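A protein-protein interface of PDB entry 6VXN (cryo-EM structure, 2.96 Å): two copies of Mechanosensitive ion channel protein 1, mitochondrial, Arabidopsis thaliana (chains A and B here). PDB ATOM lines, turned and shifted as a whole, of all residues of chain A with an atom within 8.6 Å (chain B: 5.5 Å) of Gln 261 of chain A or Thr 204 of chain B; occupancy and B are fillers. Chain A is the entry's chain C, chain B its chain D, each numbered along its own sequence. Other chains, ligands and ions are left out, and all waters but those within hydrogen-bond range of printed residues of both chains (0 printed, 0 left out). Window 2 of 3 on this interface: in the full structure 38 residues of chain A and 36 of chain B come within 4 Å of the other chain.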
ATOM      1  N   VAL A 254      -1.538   2.020  -3.544  1.00  0.00           N
ATOM      2  CA  VAL A 254      -2.788   1.413  -4.005  1.00  0.00           C
ATOM      3  C   VAL A 254      -2.513   0.213  -4.911  1.00  0.00           C
ATOM      4  O   VAL A 254      -3.276  -0.765  -4.915  1.00  0.00           O
ATOM      5  CB  VAL A 254      -3.689   2.460  -4.677  1.00  0.00           C
ATOM      6  CG1 VAL A 254      -5.066   1.907  -4.903  1.00  0.00           C
ATOM      7  CG2 VAL A 254      -3.833   3.633  -3.777  1.00  0.00           C
ATOM      8  N   LEU A 255      -1.393   0.231  -5.637  1.00  0.00           N
ATOM      9  CA  LEU A 255      -1.023  -0.917  -6.456  1.00  0.00           C
ATOM     10  C   LEU A 255      -0.714  -2.134  -5.601  1.00  0.00           C
ATOM     11  O   LEU A 255      -1.180  -3.243  -5.896  1.00  0.00           O
ATOM     12  CB  LEU A 255       0.185  -0.580  -7.325  1.00  0.00           C
ATOM     13  CG  LEU A 255      -0.064   0.014  -8.707  1.00  0.00           C
ATOM     14  CD1 LEU A 255       1.203  -0.055  -9.509  1.00  0.00           C
ATOM     15  CD2 LEU A 255      -1.190  -0.696  -9.414  1.00  0.00           C
ATOM     16  N   SER A 256       0.050  -1.949  -4.525  1.00  0.00           N
ATOM     17  CA  SER A 256       0.313  -3.079  -3.652  1.00  0.00           C
ATOM     18  C   SER A 256      -0.940  -3.491  -2.905  1.00  0.00           C
ATOM     19  O   SER A 256      -1.139  -4.679  -2.639  1.00  0.00           O
ATOM     20  CB  SER A 256       1.435  -2.747  -2.689  1.00  0.00           C
ATOM     21  OG  SER A 256       2.635  -2.554  -3.399  1.00  0.00           O
ATOM     22  N   GLY A 257      -1.824  -2.538  -2.620  1.00  0.00           N
ATOM     23  CA  GLY A 257      -3.060  -2.871  -1.946  1.00  0.00           C
ATOM     24  C   GLY A 257      -4.007  -3.686  -2.797  1.00  0.00           C
ATOM     25  O   GLY A 257      -4.847  -4.415  -2.269  1.00  0.00           O
ATOM     26  N   LEU A 258      -3.896  -3.575  -4.118  1.00  0.00           N
ATOM     27  CA  LEU A 258      -4.663  -4.466  -4.977  1.00  0.00           C
ATOM     28  C   LEU A 258      -3.962  -5.778  -5.280  1.00  0.00           C
ATOM     29  O   LEU A 258      -4.635  -6.815  -5.352  1.00  0.00           O
ATOM     30  CB  LEU A 258      -5.018  -3.784  -6.296  1.00  0.00           C
ATOM     31  CG  LEU A 258      -6.107  -2.731  -6.168  1.00  0.00           C
ATOM     32  CD1 LEU A 258      -6.105  -1.837  -7.379  1.00  0.00           C
ATOM     33  CD2 LEU A 258      -7.452  -3.396  -5.987  1.00  0.00           C
ATOM     34  N   SER A 259      -2.639  -5.767  -5.454  1.00  0.00           N
ATOM     35  CA  SER A 259      -1.942  -7.018  -5.723  1.00  0.00           C
ATOM     36  C   SER A 259      -1.982  -7.949  -4.522  1.00  0.00           C
ATOM     37  O   SER A 259      -2.003  -9.170  -4.689  1.00  0.00           O
ATOM     38  CB  SER A 259      -0.500  -6.758  -6.126  1.00  0.00           C
ATOM     39  OG  SER A 259       0.175  -7.978  -6.340  1.00  0.00           O
ATOM     40  N   MET A 260      -2.029  -7.404  -3.312  1.00  0.00           N
ATOM     41  CA  MET A 260      -2.292  -8.243  -2.158  1.00  0.00           C
ATOM     42  C   MET A 260      -3.732  -8.699  -2.087  1.00  0.00           C
ATOM     43  O   MET A 260      -4.015  -9.683  -1.404  1.00  0.00           O
ATOM     44  CB  MET A 260      -1.955  -7.507  -0.874  1.00  0.00           C
ATOM     45  CG  MET A 260      -0.492  -7.310  -0.639  1.00  0.00           C
ATOM     46  SD  MET A 260      -0.216  -6.845   1.066  1.00  0.00           S
ATOM     47  CE  MET A 260      -1.520  -5.655   1.323  1.00  0.00           C
ATOM     48  N   GLN A 261      -4.648  -8.010  -2.742  1.00  0.00           N
ATOM     49  CA  GLN A 261      -6.022  -8.471  -2.759  1.00  0.00           C
ATOM     50  C   GLN A 261      -6.245  -9.585  -3.752  1.00  0.00           C
ATOM     51  O   GLN A 261      -7.153 -10.397  -3.558  1.00  0.00           O
ATOM     52  CB  GLN A 261      -6.972  -7.325  -3.077  1.00  0.00           C
ATOM     53  CG  GLN A 261      -7.449  -6.599  -1.859  1.00  0.00           C
ATOM     54  CD  GLN A 261      -8.300  -7.472  -0.977  1.00  0.00           C
ATOM     55  OE1 GLN A 261      -9.056  -8.307  -1.464  1.00  0.00           O
ATOM     56  NE2 GLN A 261      -8.190  -7.280   0.329  1.00  0.00           N
ATOM     57  N   PHE A 262      -5.453  -9.641  -4.812  1.00  0.00           N
ATOM     58  CA  PHE A 262      -5.607 -10.762  -5.727  1.00  0.00           C
ATOM     59  C   PHE A 262      -4.917 -11.995  -5.174  1.00  0.00           C
ATOM     60  O   PHE A 262      -5.574 -12.987  -4.855  1.00  0.00           O
ATOM     61  CB  PHE A 262      -5.056 -10.418  -7.104  1.00  0.00           C
ATOM     62  CG  PHE A 262      -5.958  -9.540  -7.908  1.00  0.00           C
ATOM     63  CD1 PHE A 262      -7.283  -9.356  -7.533  1.00  0.00           C
ATOM     64  CD2 PHE A 262      -5.484  -8.889  -9.033  1.00  0.00           C
ATOM     65  CE1 PHE A 262      -8.118  -8.542  -8.267  1.00  0.00           C
ATOM     66  CE2 PHE A 262      -6.314  -8.075  -9.772  1.00  0.00           C
ATOM     67  CZ  PHE A 262      -7.633  -7.902  -9.389  1.00  0.00           C
ATOM     68  N   SER A 263      -3.599 -11.936  -5.022  1.00  0.00           N
ATOM     69  CA  SER A 263      -2.816 -13.095  -4.614  1.00  0.00           C
ATOM     70  C   SER A 263      -2.569 -13.003  -3.115  1.00  0.00           C
ATOM     71  O   SER A 263      -1.528 -12.546  -2.671  1.00  0.00           O
ATOM     72  CB  SER A 263      -1.513 -13.149  -5.394  1.00  0.00           C
ATOM     73  OG  SER A 263      -0.690 -12.037  -5.106  1.00  0.00           O
ATOM     74  N   ARG A 264      -3.537 -13.483  -2.339  1.00  0.00           N
ATOM     75  CA  ARG A 264      -3.640 -13.189  -0.911  1.00  0.00           C
ATOM     76  C   ARG A 264      -2.514 -13.804  -0.096  1.00  0.00           C
ATOM     77  O   ARG A 264      -2.459 -15.032   0.027  1.00  0.00           O
ATOM     78  CB  ARG A 264      -4.957 -13.718  -0.387  1.00  0.00           C
ATOM     79  CG  ARG A 264      -6.138 -13.255  -1.162  1.00  0.00           C
ATOM     80  CD  ARG A 264      -7.398 -13.761  -0.516  1.00  0.00           C
ATOM     81  NE  ARG A 264      -8.541 -12.927  -0.863  1.00  0.00           N
ATOM     82  CZ  ARG A 264      -8.915 -11.859  -0.168  1.00  0.00           C
ATOM     83  NH1 ARG A 264      -8.234 -11.500   0.913  1.00  0.00           N
ATOM     84  NH2 ARG A 264      -9.969 -11.149  -0.550  1.00  0.00           N
ATOM     85  N   PRO A 265      -1.637 -13.018   0.496  1.00  0.00           N
ATOM     86  CA  PRO A 265      -0.601 -13.612   1.336  1.00  0.00           C
ATOM     87  C   PRO A 265      -1.059 -13.815   2.765  1.00  0.00           C
ATOM     88  O   PRO A 265      -0.491 -14.642   3.479  1.00  0.00           O
ATOM     89  CB  PRO A 265       0.536 -12.598   1.242  1.00  0.00           C
ATOM     90  CG  PRO A 265      -0.125 -11.331   1.009  1.00  0.00           C
ATOM     91  CD  PRO A 265      -1.447 -11.569   0.355  1.00  0.00           C
ATOM     92  N   PHE A 266      -2.252 -13.188   3.332  1.00  0.00           N
ATOM     93  CA  PHE A 266      -2.779 -13.313   4.682  1.00  0.00           C
ATOM     94  C   PHE A 266      -4.224 -12.845   4.683  1.00  0.00           C
ATOM     95  O   PHE A 266      -4.720 -12.290   3.701  1.00  0.00           O
ATOM     96  CB  PHE A 266      -1.942 -12.527   5.698  1.00  0.00           C
ATOM     97  CG  PHE A 266      -1.554 -11.146   5.248  1.00  0.00           C
ATOM     98  CD1 PHE A 266      -2.437 -10.085   5.347  1.00  0.00           C
ATOM     99  CD2 PHE A 266      -0.293 -10.909   4.742  1.00  0.00           C
ATOM    100  CE1 PHE A 266      -2.073  -8.826   4.938  1.00  0.00           C
ATOM    101  CE2 PHE A 266       0.072  -9.648   4.334  1.00  0.00           C
ATOM    102  CZ  PHE A 266      -0.820  -8.610   4.432  1.00  0.00           C
ATOM    103  N   SER A 267      -4.895 -13.073   5.804  1.00  0.00           N
ATOM    104  CA  SER A 267      -6.279 -12.671   5.975  1.00  0.00           C
ATOM    105  C   SER A 267      -6.411 -11.971   7.318  1.00  0.00           C
ATOM    106  O   SER A 267      -5.442 -11.839   8.067  1.00  0.00           O
ATOM    107  CB  SER A 267      -7.224 -13.868   5.882  1.00  0.00           C
ATOM    108  OG  SER A 267      -7.196 -14.422   4.580  1.00  0.00           O
ATOM    109  N   MET A 268      -7.622 -11.504   7.609  1.00  0.00           N
ATOM    110  CA  MET A 268      -7.887 -10.786   8.850  1.00  0.00           C
ATOM    111  C   MET A 268      -7.790 -11.730  10.040  1.00  0.00           C
ATOM    112  O   MET A 268      -8.489 -12.747  10.094  1.00  0.00           O
ATOM    113  CB  MET A 268      -9.265 -10.138   8.795  1.00  0.00           C
ATOM    114  CG  MET A 268      -9.299  -8.806   8.082  1.00  0.00           C
ATOM    115  SD  MET A 268      -8.962  -7.450   9.207  1.00  0.00           S
ATOM    116  CE  MET A 268     -10.242  -7.725  10.423  1.00  0.00           C
ATOM    117  N   MET A 284      -7.224  -4.612   7.182  1.00  0.00           N
ATOM    118  CA  MET A 284      -6.652  -4.551   5.842  1.00  0.00           C
ATOM    119  C   MET A 284      -7.329  -3.411   5.095  1.00  0.00           C
ATOM    120  O   MET A 284      -8.509  -3.507   4.744  1.00  0.00           O
ATOM    121  CB  MET A 284      -6.834  -5.873   5.105  1.00  0.00           C
ATOM    122  CG  MET A 284      -6.243  -7.063   5.819  1.00  0.00           C
ATOM    123  SD  MET A 284      -6.305  -8.578   4.854  1.00  0.00           S
ATOM    124  CE  MET A 284      -5.529  -8.037   3.338  1.00  0.00           C
ATOM    125  N   GLY A 285      -6.587  -2.334   4.850  1.00  0.00           N
ATOM    126  CA  GLY A 285      -7.127  -1.137   4.251  1.00  0.00           C
ATOM    127  C   GLY A 285      -6.699  -0.954   2.804  1.00  0.00           C
ATOM    128  O   GLY A 285      -6.051  -1.800   2.194  1.00  0.00           O
ATOM    129  N   LEU A 286      -7.087   0.200   2.262  1.00  0.00           N
ATOM    130  CA  LEU A 286      -6.820   0.490   0.857  1.00  0.00           C
ATOM    131  C   LEU A 286      -5.382   0.947   0.639  1.00  0.00           C
ATOM    132  O   LEU A 286      -4.754   0.563  -0.352  1.00  0.00           O
ATOM    133  CB  LEU A 286      -7.818   1.530   0.324  1.00  0.00           C
ATOM    134  CG  LEU A 286      -7.804   3.024   0.686  1.00  0.00           C
ATOM    135  CD1 LEU A 286      -8.571   3.823  -0.349  1.00  0.00           C
ATOM    136  CD2 LEU A 286      -8.384   3.287   2.069  1.00  0.00           C
ATOM    137  N   ASN A 303       1.032  -0.336   2.441  1.00  0.00           N
ATOM    138  CA  ASN A 303       0.922  -1.563   1.650  1.00  0.00           C
ATOM    139  C   ASN A 303       2.145  -1.824   0.787  1.00  0.00           C
ATOM    140  O   ASN A 303       2.489  -2.979   0.524  1.00  0.00           O
ATOM    141  CB  ASN A 303      -0.312  -1.524   0.758  1.00  0.00           C
ATOM    142  CG  ASN A 303      -1.582  -1.742   1.516  1.00  0.00           C
ATOM    143  OD1 ASN A 303      -2.545  -1.009   1.355  1.00  0.00           O
ATOM    144  ND2 ASN A 303      -1.590  -2.753   2.369  1.00  0.00           N
ATOM    145  N   GLU B 200     -14.576 -12.033   2.516  1.00  0.00           N
ATOM    146  CA  GLU B 200     -13.445 -11.530   1.749  1.00  0.00           C
ATOM    147  C   GLU B 200     -13.909 -10.924   0.433  1.00  0.00           C
ATOM    148  O   GLU B 200     -13.265 -10.001  -0.090  1.00  0.00           O
ATOM    149  CB  GLU B 200     -12.450 -12.657   1.488  1.00  0.00           C
ATOM    150  CG  GLU B 200     -12.354 -13.670   2.615  1.00  0.00           C
ATOM    151  CD  GLU B 200     -13.193 -14.913   2.358  1.00  0.00           C
ATOM    152  OE1 GLU B 200     -14.437 -14.815   2.391  1.00  0.00           O
ATOM    153  OE2 GLU B 200     -12.607 -15.989   2.116  1.00  0.00           O
ATOM    154  N   LYS B 201     -15.024 -11.432  -0.102  1.00  0.00           N
ATOM    155  CA  LYS B 201     -15.606 -10.871  -1.314  1.00  0.00           C
ATOM    156  C   LYS B 201     -16.073  -9.442  -1.084  1.00  0.00           C
ATOM    157  O   LYS B 201     -15.933  -8.593  -1.967  1.00  0.00           O
ATOM    158  CB  LYS B 201     -16.768 -11.738  -1.792  1.00  0.00           C
ATOM    159  CG  LYS B 201     -16.467 -13.227  -1.815  1.00  0.00           C
ATOM    160  CD  LYS B 201     -17.744 -14.031  -2.006  1.00  0.00           C
ATOM    161  CE  LYS B 201     -17.491 -15.527  -1.896  1.00  0.00           C
ATOM    162  NZ  LYS B 201     -18.753 -16.307  -2.031  1.00  0.00           N
ATOM    163  N   VAL B 202     -16.586  -9.158   0.117  1.00  0.00           N
ATOM    164  CA  VAL B 202     -16.990  -7.804   0.489  1.00  0.00           C
ATOM    165  C   VAL B 202     -15.796  -6.862   0.466  1.00  0.00           C
ATOM    166  O   VAL B 202     -15.872  -5.755  -0.084  1.00  0.00           O
ATOM    167  CB  VAL B 202     -17.671  -7.829   1.870  1.00  0.00           C
ATOM    168  CG1 VAL B 202     -17.871  -6.428   2.410  1.00  0.00           C
ATOM    169  CG2 VAL B 202     -18.997  -8.551   1.778  1.00  0.00           C
ATOM    170  N   LEU B 203     -14.661  -7.309   1.010  1.00  0.00           N
ATOM    171  CA  LEU B 203     -13.490  -6.447   1.102  1.00  0.00           C
ATOM    172  C   LEU B 203     -12.869  -6.195  -0.265  1.00  0.00           C
ATOM    173  O   LEU B 203     -12.563  -5.042  -0.604  1.00  0.00           O
ATOM    174  CB  LEU B 203     -12.459  -7.053   2.050  1.00  0.00           C
ATOM    175  CG  LEU B 203     -12.787  -7.245   3.535  1.00  0.00           C
ATOM    176  CD1 LEU B 203     -11.508  -7.131   4.348  1.00  0.00           C
ATOM    177  CD2 LEU B 203     -13.816  -6.244   4.053  1.00  0.00           C
ATOM    178  N   THR B 204     -12.712  -7.241  -1.084  1.00  0.00           N
ATOM    179  CA  THR B 204     -12.163  -7.001  -2.416  1.00  0.00           C
ATOM    180  C   THR B 204     -13.141  -6.215  -3.280  1.00  0.00           C
ATOM    181  O   THR B 204     -12.714  -5.375  -4.082  1.00  0.00           O
ATOM    182  CB  THR B 204     -11.748  -8.313  -3.094  1.00  0.00           C
ATOM    183  OG1 THR B 204     -11.153  -8.025  -4.365  1.00  0.00           O
ATOM    184  CG2 THR B 204     -12.911  -9.260  -3.300  1.00  0.00           C
ATOM    185  N   LEU B 205     -14.447  -6.370  -3.029  1.00  0.00           N
ATOM    186  CA  LEU B 205     -15.449  -5.685  -3.827  1.00  0.00           C
ATOM    187  C   LEU B 205     -15.470  -4.197  -3.530  1.00  0.00           C
ATOM    188  O   LEU B 205     -15.448  -3.380  -4.453  1.00  0.00           O
ATOM    189  CB  LEU B 205     -16.821  -6.306  -3.578  1.00  0.00           C
ATOM    190  CG  LEU B 205     -17.937  -5.934  -4.550  1.00  0.00           C
ATOM    191  CD1 LEU B 205     -18.624  -7.185  -5.083  1.00  0.00           C
ATOM    192  CD2 LEU B 205     -18.943  -5.023  -3.869  1.00  0.00           C
ATOM    193  N   ASP B 206     -15.484  -3.812  -2.255  1.00  0.00           N
ATOM    194  CA  ASP B 206     -15.555  -2.380  -1.988  1.00  0.00           C
ATOM    195  C   ASP B 206     -14.189  -1.713  -2.156  1.00  0.00           C
ATOM    196  O   ASP B 206     -14.116  -0.504  -2.393  1.00  0.00           O
ATOM    197  CB  ASP B 206     -16.196  -2.088  -0.621  1.00  0.00           C
ATOM    198  CG  ASP B 206     -15.504  -2.754   0.553  1.00  0.00           C
ATOM    199  OD1 ASP B 206     -14.356  -3.209   0.450  1.00  0.00           O
ATOM    200  OD2 ASP B 206     -16.127  -2.795   1.629  1.00  0.00           O
ATOM    201  N   LYS B 207     -13.100  -2.496  -2.143  1.00  0.00           N
ATOM    202  CA  LYS B 207     -11.816  -1.904  -2.517  1.00  0.00           C
ATOM    203  C   LYS B 207     -11.746  -1.595  -4.012  1.00  0.00           C
ATOM    204  O   LYS B 207     -11.330  -0.489  -4.402  1.00  0.00           O
ATOM    205  CB  LYS B 207     -10.672  -2.816  -2.104  1.00  0.00           C
ATOM    206  CG  LYS B 207     -10.299  -2.677  -0.647  1.00  0.00           C
ATOM    207  CD  LYS B 207      -9.008  -3.404  -0.350  1.00  0.00           C
ATOM    208  CE  LYS B 207      -8.770  -3.511   1.142  1.00  0.00           C
ATOM    209  NZ  LYS B 207      -9.873  -4.222   1.834  1.00  0.00           N
ATOM    210  N   VAL B 208     -12.164  -2.540  -4.867  1.00  0.00           N
ATOM    211  CA  VAL B 208     -12.120  -2.239  -6.297  1.00  0.00           C
ATOM    212  C   VAL B 208     -13.204  -1.231  -6.657  1.00  0.00           C
ATOM    213  O   VAL B 208     -13.039  -0.451  -7.599  1.00  0.00           O
ATOM    214  CB  VAL B 208     -12.225  -3.505  -7.173  1.00  0.00           C
ATOM    215  CG1 VAL B 208     -11.006  -4.398  -6.987  1.00  0.00           C
ATOM    216  CG2 VAL B 208     -13.534  -4.248  -6.983  1.00  0.00           C
ATOM    217  N   SER B 209     -14.290  -1.177  -5.884  1.00  0.00           N
ATOM    218  CA  SER B 209     -15.298  -0.146  -6.067  1.00  0.00           C
ATOM    219  C   SER B 209     -14.808   1.233  -5.659  1.00  0.00           C
ATOM    220  O   SER B 209     -15.169   2.210  -6.315  1.00  0.00           O
ATOM    221  CB  SER B 209     -16.548  -0.494  -5.265  1.00  0.00           C
ATOM    222  OG  SER B 209     -16.522   0.175  -4.021  1.00  0.00           O
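NH2 of Arg 264 of chain A lies within hydrogen-bond range of OE1 of Gln 261 of chain A (3.1 Å).
Gln 261 of chain A touches just these residues of chain B: Thr 204 and Lys 207.
Of the printed residues of chain B, Gly 285 of chain A touches Lys 207.
Of the printed residues of chain A, Val 208 of chain B touches Leu 258.
Of the printed residues of chain A, Glu 200 of chain B touches Arg 264 (3.5 Å).
Printed residues of chain A within 4 Å of Lys 207 of chain B: Gln 261, Met 284 and Gly 285.
Leu 255 of chain A touches none of the printed residues of chain B.
Ser 256 of chain A touches none of the printed residues of chain B.
The nearest residue of chain B that does not touch Gln 261 of chain A is Leu 203 of chain B (4.5 Å).
The nearest printed residue of chain A that does not touch Lys 207 of chain B is Leu 286 of chain A (4.2 Å).
Leu 258 of chain A touches Val 208 of chain B.
Gln 261 of chain A touches Thr 204 of chain B.
Gln 261 of chain A touches Lys 207 of chain B.
Arg 264 of chain A touches Glu 200 of chain B (NH2 to O, 3.5 Å).
Gly 285 of chain A touches Lys 207 of chain B (O to CE, 3.4 Å).
The side-chain amino group (NZ) of Lys 207 of chain B is in hydrogen-bond range of the backbone carbonyl oxygen (O) of Met 284 of chain A, 3.3 Å away.
Along chain A the printed residues that touch a printed residue of chain B span positions 258 to 285.
Among the printed residues, no Asp or Glu carboxylate lies within 4 Å of a Lys or Arg side-chain nitrogen of the other chain.
No position is printed for both chains.
Of the 6 pairs that touch across the chains among the printed residues, none has its exchanged pair printed and touching as well.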
